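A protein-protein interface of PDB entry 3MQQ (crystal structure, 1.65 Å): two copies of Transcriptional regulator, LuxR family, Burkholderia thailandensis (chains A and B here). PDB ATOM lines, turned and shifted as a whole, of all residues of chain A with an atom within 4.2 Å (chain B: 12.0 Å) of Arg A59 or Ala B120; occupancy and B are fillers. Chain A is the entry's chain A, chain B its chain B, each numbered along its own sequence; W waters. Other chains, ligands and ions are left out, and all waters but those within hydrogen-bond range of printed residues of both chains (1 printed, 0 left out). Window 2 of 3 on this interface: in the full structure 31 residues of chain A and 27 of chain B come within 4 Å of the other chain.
The backbone carbonyl oxygen (O) of Asp A77 sits at hydrogen-bond distance from the backbone NH (N) of Ala B120 (2.9 Å).
The side-chain carboxylate (OD2) of Asp A77 lies within salt-bridge range of the guanidinium group (NE) of Arg B117, 2.8 Å away.
The guanidinium group (NH1) of Arg A63 is in hydrogen-bond range of the backbone carbonyl oxygen (O) of Val B119 (3.3 Å).
The backbone NH (N) of Asp A77 sits at hydrogen-bond distance from the backbone carbonyl oxygen (O) of Arg B118, at 2.9 Å.
The side-chain carboxylate (OD1) of Asp A76 lies within salt-bridge range of the guanidinium group (NE) of Arg A78 (2.7 Å).
The guanidinium group (NE) of Arg A59 is in salt-bridge range of the side-chain carboxylate (OE2) of Glu A56.
Among the printed residues, pairs that only touch across the chains: Arg A59 with Ala B120, Arg A63 with Arg B118, Arg A63 with Ala B120, Asp A76 with Arg B118, Asp A76 with Ala B120, Asp A77 with Val B119 and Arg A78 with Ala B120.
No residue of chain B comes within 4 Å of Glu A56.
Phe A57 touches none of the printed residues of chain B.
No residue of chain B comes within 4 Å of Glu A58.
Of chain B, only Ala B120 comes within 4 Å of Arg A59.
No residue of chain B comes within 4 Å of Glu A62.
Of chain B, only Arg B118 (3.5 Å), Val B119 (3.3 Å) and Ala B120 (3.7 Å) come within 4 Å of Arg A63.
Printed residues of chain B within 4 Å of Asp A76: Arg B118 (3.0 Å) and Ala B120 (3.4 Å).
Of chain B, only Arg B117, Arg B118, Val B119 and Ala B120 come within 4 Å of Asp A77.
Of chain B, only Ala B120 (3.5 Å) comes within 4 Å of Arg A78.
Printed residues of chain A within 4 Å of Arg B117: Asp A77 (2.8 Å).
Of the printed residues of chain A, Val B119 touches Arg A63 (3.3 Å) and Asp A77 (3.6 Å).
Of chain A, only Arg A59, Arg A63, Asp A76, Asp A77 and Arg A78 come within 4 Å of Ala B120.
The nearest residue of chain B that does not touch Arg A59 is Val B119 (6.1 Å).
The nearest printed residue of chain A that does not touch Val B119 is Asp A76 (4.8 Å).
Of the 12 printed residues of chain A, 5 touch a printed residue of chain B.
Of the 5 printed residues of chain B, 4 touch a printed residue of chain A.
Printed residues of chain B that touch a printed residue of chain A: Arg B117, Arg B118, Val B119 and Ala B120.
Among the printed residues, 11 pairs touch across the chains.
Among the printed residues, Asp or Glu carboxylates within 4 Å of a Lys or Arg side-chain nitrogen of the other chain: Asp A77 with Arg B117.
No position is printed for both chains.
Of the 11 pairs that touch across the chains among the printed residues, none has its exchanged pair printed and touching as well.
Water W1 lies within hydrogen-bond range of the side-chain carboxylate (OD2) of Asp A77 (3.2 Å) and the backbone carbonyl oxygen (O) of Arg B118 (3.4 Å).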
ATOM      1  N   ASP A  55       2.923 -19.057  11.793  1.00  0.00           N
ATOM      2  CA  ASP A  55       3.468 -18.814  10.461  1.00  0.00           C
ATOM      3  C   ASP A  55       4.996 -18.859  10.418  1.00  0.00           C
ATOM      4  O   ASP A  55       5.579 -19.422   9.483  1.00  0.00           O
ATOM      5  CB  ASP A  55       2.975 -17.489   9.907  1.00  0.00           C
ATOM      6  CG  ASP A  55       1.546 -17.569   9.364  1.00  0.00           C
ATOM      7  OD1 ASP A  55       0.949 -18.676   9.394  1.00  0.00           O
ATOM      8  OD2 ASP A  55       1.031 -16.528   8.900  1.00  0.00           O
ATOM      9  N   GLU A  56       5.638 -18.258  11.418  1.00  0.00           N
ATOM     10  CA  GLU A  56       7.107 -18.304  11.513  1.00  0.00           C
ATOM     11  C   GLU A  56       7.625 -19.715  11.764  1.00  0.00           C
ATOM     12  O   GLU A  56       8.600 -20.138  11.161  1.00  0.00           O
ATOM     13  CB  GLU A  56       7.645 -17.319  12.559  1.00  0.00           C
ATOM     14  CG  GLU A  56       7.540 -15.829  12.155  1.00  0.00           C
ATOM     15  CD  GLU A  56       8.406 -15.445  10.966  1.00  0.00           C
ATOM     16  OE1 GLU A  56       9.372 -14.676  11.160  1.00  0.00           O
ATOM     17  OE2 GLU A  56       8.112 -15.881   9.831  1.00  0.00           O
ATOM     18  N   PHE A  57       6.954 -20.446  12.647  1.00  0.00           N
ATOM     19  CA  PHE A  57       7.300 -21.843  12.910  1.00  0.00           C
ATOM     20  C   PHE A  57       7.261 -22.658  11.605  1.00  0.00           C
ATOM     21  O   PHE A  57       8.169 -23.460  11.344  1.00  0.00           O
ATOM     22  CB  PHE A  57       6.320 -22.391  13.941  1.00  0.00           C
ATOM     23  CG  PHE A  57       6.343 -23.881  14.091  1.00  0.00           C
ATOM     24  CD1 PHE A  57       7.424 -24.515  14.690  1.00  0.00           C
ATOM     25  CD2 PHE A  57       5.256 -24.656  13.652  1.00  0.00           C
ATOM     26  CE1 PHE A  57       7.418 -25.895  14.864  1.00  0.00           C
ATOM     27  CE2 PHE A  57       5.236 -26.030  13.814  1.00  0.00           C
ATOM     28  CZ  PHE A  57       6.327 -26.675  14.421  1.00  0.00           C
ATOM     29  N   GLU A  58       6.230 -22.418  10.788  1.00  0.00           N
ATOM     30  CA  GLU A  58       6.072 -23.123   9.497  1.00  0.00           C
ATOM     31  C   GLU A  58       7.135 -22.697   8.471  1.00  0.00           C
ATOM     32  O   GLU A  58       7.719 -23.536   7.797  1.00  0.00           O
ATOM     33  CB  GLU A  58       4.658 -22.901   8.927  1.00  0.00           C
ATOM     34  N   ARG A  59       7.391 -21.390   8.385  1.00  0.00           N
ATOM     35  CA  ARG A  59       8.300 -20.822   7.395  1.00  0.00           C
ATOM     36  C   ARG A  59       9.725 -21.274   7.656  1.00  0.00           C
ATOM     37  O   ARG A  59      10.446 -21.682   6.736  1.00  0.00           O
ATOM     38  CB  ARG A  59       8.194 -19.281   7.388  1.00  0.00           C
ATOM     39  CG  ARG A  59       9.099 -18.572   6.357  1.00  0.00           C
ATOM     40  CD  ARG A  59       9.105 -17.039   6.499  1.00  0.00           C
ATOM     41  NE  ARG A  59       9.795 -16.542   7.699  1.00  0.00           N
ATOM     42  CZ  ARG A  59      11.109 -16.336   7.794  1.00  0.00           C
ATOM     43  NH1 ARG A  59      11.917 -16.597   6.772  1.00  0.00           N
ATOM     44  NH2 ARG A  59      11.625 -15.867   8.926  1.00  0.00           N
ATOM     45  N   ILE A  60      10.129 -21.221   8.923  1.00  0.00           N
ATOM     46  CA  ILE A  60      11.492 -21.565   9.283  1.00  0.00           C
ATOM     47  C   ILE A  60      11.733 -23.085   9.189  1.00  0.00           C
ATOM     48  O   ILE A  60      12.832 -23.523   8.839  1.00  0.00           O
ATOM     49  CB  ILE A  60      11.908 -20.883  10.629  1.00  0.00           C
ATOM     50  CG1 ILE A  60      12.016 -19.360  10.393  1.00  0.00           C
ATOM     51  CG2 ILE A  60      13.242 -21.402  11.140  1.00  0.00           C
ATOM     52  CD1 ILE A  60      12.106 -18.499  11.663  1.00  0.00           C
ATOM     53  N   GLY A  61      10.693 -23.873   9.449  1.00  0.00           N
ATOM     54  CA  GLY A  61      10.759 -25.326   9.256  1.00  0.00           C
ATOM     55  C   GLY A  61      11.038 -25.653   7.791  1.00  0.00           C
ATOM     56  O   GLY A  61      11.820 -26.541   7.479  1.00  0.00           O
ATOM     57  N   GLU A  62      10.396 -24.927   6.883  1.00  0.00           N
ATOM     58  CA  GLU A  62      10.641 -25.124   5.460  1.00  0.00           C
ATOM     59  C   GLU A  62      12.034 -24.646   5.037  1.00  0.00           C
ATOM     60  O   GLU A  62      12.579 -25.098   4.028  1.00  0.00           O
ATOM     61  CB  GLU A  62       9.532 -24.459   4.644  1.00  0.00           C
ATOM     62  CG  GLU A  62       8.215 -25.222   4.725  1.00  0.00           C
ATOM     63  CD  GLU A  62       7.116 -24.605   3.893  1.00  0.00           C
ATOM     64  OE1 GLU A  62       7.431 -23.910   2.897  1.00  0.00           O
ATOM     65  OE2 GLU A  62       5.926 -24.824   4.220  1.00  0.00           O
ATOM     66  N   ARG A  63      12.614 -23.743   5.819  1.00  0.00           N
ATOM     67  CA  ARG A  63      13.980 -23.286   5.585  1.00  0.00           C
ATOM     68  C   ARG A  63      15.007 -24.298   6.109  1.00  0.00           C
ATOM     69  O   ARG A  63      16.040 -24.530   5.475  1.00  0.00           O
ATOM     70  CB  ARG A  63      14.177 -21.896   6.215  1.00  0.00           C
ATOM     71  CG  ARG A  63      15.565 -21.291   6.072  1.00  0.00           C
ATOM     72  CD  ARG A  63      15.726 -20.548   4.755  1.00  0.00           C
ATOM     73  NE  ARG A  63      16.974 -19.787   4.701  1.00  0.00           N
ATOM     74  CZ  ARG A  63      17.093 -18.508   5.055  1.00  0.00           C
ATOM     75  NH1 ARG A  63      18.270 -17.904   4.968  1.00  0.00           N
ATOM     76  NH2 ARG A  63      16.039 -17.832   5.493  1.00  0.00           N
ATOM     77  N   ASP A  76      21.261 -20.534  12.249  1.00  0.00           N
ATOM     78  CA  ASP A  76      20.753 -19.256  11.786  1.00  0.00           C
ATOM     79  C   ASP A  76      20.572 -18.335  12.973  1.00  0.00           C
ATOM     80  O   ASP A  76      20.806 -18.729  14.096  1.00  0.00           O
ATOM     81  CB  ASP A  76      19.427 -19.437  11.032  1.00  0.00           C
ATOM     82  CG  ASP A  76      18.259 -19.745  11.939  1.00  0.00           C
ATOM     83  OD1 ASP A  76      18.333 -19.411  13.138  1.00  0.00           O
ATOM     84  OD2 ASP A  76      17.236 -20.284  11.431  1.00  0.00           O
ATOM     85  N   ASP A  77      20.169 -17.111  12.693  1.00  0.00           N
ATOM     86  CA  ASP A  77      19.731 -16.194  13.713  1.00  0.00           C
ATOM     87  C   ASP A  77      18.299 -15.917  13.340  1.00  0.00           C
ATOM     88  O   ASP A  77      17.978 -15.796  12.144  1.00  0.00           O
ATOM     89  CB  ASP A  77      20.553 -14.911  13.645  1.00  0.00           C
ATOM     90  CG  ASP A  77      22.004 -15.166  13.867  1.00  0.00           C
ATOM     91  OD1 ASP A  77      22.324 -15.915  14.846  1.00  0.00           O
ATOM     92  OD2 ASP A  77      22.819 -14.709  13.049  1.00  0.00           O
ATOM     93  N   ARG A  78      17.433 -15.876  14.337  1.00  0.00           N
ATOM     94  CA  ARG A  78      16.028 -15.514  14.091  1.00  0.00           C
ATOM     95  C   ARG A  78      15.384 -14.892  15.299  1.00  0.00           C
ATOM     96  O   ARG A  78      15.864 -15.024  16.426  1.00  0.00           O
ATOM     97  CB  ARG A  78      15.208 -16.707  13.607  1.00  0.00           C
ATOM     98  CG  ARG A  78      14.573 -17.570  14.732  1.00  0.00           C
ATOM     99  CD  ARG A  78      15.646 -18.447  15.439  1.00  0.00           C
ATOM    100  NE  ARG A  78      16.044 -19.578  14.596  1.00  0.00           N
ATOM    101  CZ  ARG A  78      15.400 -20.746  14.517  1.00  0.00           C
ATOM    102  NH1 ARG A  78      14.303 -20.970  15.226  1.00  0.00           N
ATOM    103  NH2 ARG A  78      15.844 -21.682  13.696  1.00  0.00           N
ATOM    104  N   THR B 116      29.599 -17.134   6.777  1.00  0.00           N
ATOM    105  CA  THR B 116      28.564 -16.097   6.782  1.00  0.00           C
ATOM    106  C   THR B 116      27.374 -16.625   7.592  1.00  0.00           C
ATOM    107  O   THR B 116      26.961 -17.780   7.421  1.00  0.00           O
ATOM    108  CB  THR B 116      28.100 -15.743   5.342  1.00  0.00           C
ATOM    109  OG1 THR B 116      29.215 -15.271   4.566  1.00  0.00           O
ATOM    110  CG2 THR B 116      27.018 -14.655   5.354  1.00  0.00           C
ATOM    111  N   ARG B 117      26.852 -15.782   8.481  1.00  0.00           N
ATOM    112  CA  ARG B 117      25.709 -16.133   9.318  1.00  0.00           C
ATOM    113  C   ARG B 117      24.431 -16.137   8.484  1.00  0.00           C
ATOM    114  O   ARG B 117      24.116 -15.155   7.784  1.00  0.00           O
ATOM    115  CB  ARG B 117      25.557 -15.141  10.475  1.00  0.00           C
ATOM    116  CG  ARG B 117      26.733 -15.117  11.429  1.00  0.00           C
ATOM    117  CD  ARG B 117      26.482 -14.178  12.587  1.00  0.00           C
ATOM    118  NE  ARG B 117      25.588 -14.778  13.565  1.00  0.00           N
ATOM    119  CZ  ARG B 117      26.010 -15.488  14.599  1.00  0.00           C
ATOM    120  NH1 ARG B 117      25.137 -15.999  15.455  1.00  0.00           N
ATOM    121  NH2 ARG B 117      27.311 -15.677  14.785  1.00  0.00           N
ATOM    122  N   ARG B 118      23.696 -17.239   8.586  1.00  0.00           N
ATOM    123  CA  ARG B 118      22.412 -17.372   7.926  1.00  0.00           C
ATOM    124  C   ARG B 118      21.401 -16.665   8.802  1.00  0.00           C
ATOM    125  O   ARG B 118      21.355 -16.881  10.013  1.00  0.00           O
ATOM    126  CB  ARG B 118      22.049 -18.855   7.771  1.00  0.00           C
ATOM    127  CG  ARG B 118      20.643 -19.104   7.226  1.00  0.00           C
ATOM    128  CD  ARG B 118      20.316 -20.601   7.127  1.00  0.00           C
ATOM    129  NE  ARG B 118      21.059 -21.252   6.047  1.00  0.00           N
ATOM    130  CZ  ARG B 118      22.112 -22.053   6.215  1.00  0.00           C
ATOM    131  NH1 ARG B 118      22.577 -22.324   7.436  1.00  0.00           N
ATOM    132  NH2 ARG B 118      22.702 -22.596   5.156  1.00  0.00           N
ATOM    133  N   VAL B 119      20.618 -15.785   8.200  1.00  0.00           N
ATOM    134  CA  VAL B 119      19.561 -15.143   8.941  1.00  0.00           C
ATOM    135  C   VAL B 119      18.216 -15.624   8.419  1.00  0.00           C
ATOM    136  O   VAL B 119      17.922 -15.507   7.230  1.00  0.00           O
ATOM    137  CB  VAL B 119      19.675 -13.600   8.893  1.00  0.00           C
ATOM    138  CG1 VAL B 119      18.497 -12.964   9.638  1.00  0.00           C
ATOM    139  CG2 VAL B 119      21.024 -13.152   9.513  1.00  0.00           C
ATOM    140  N   ALA B 120      17.416 -16.187   9.318  1.00  0.00           N
ATOM    141  CA  ALA B 120      16.037 -16.553   9.000  1.00  0.00           C
ATOM    142  C   ALA B 120      15.083 -15.469   9.507  1.00  0.00           C
ATOM    143  O   ALA B 120      15.280 -14.904  10.595  1.00  0.00           O
ATOM    144  CB  ALA B 120      15.697 -17.898   9.612  1.00  0.00           C
HETATM  145  O   HOH W   1      23.785 -17.692  12.197  1.00  0.00           O
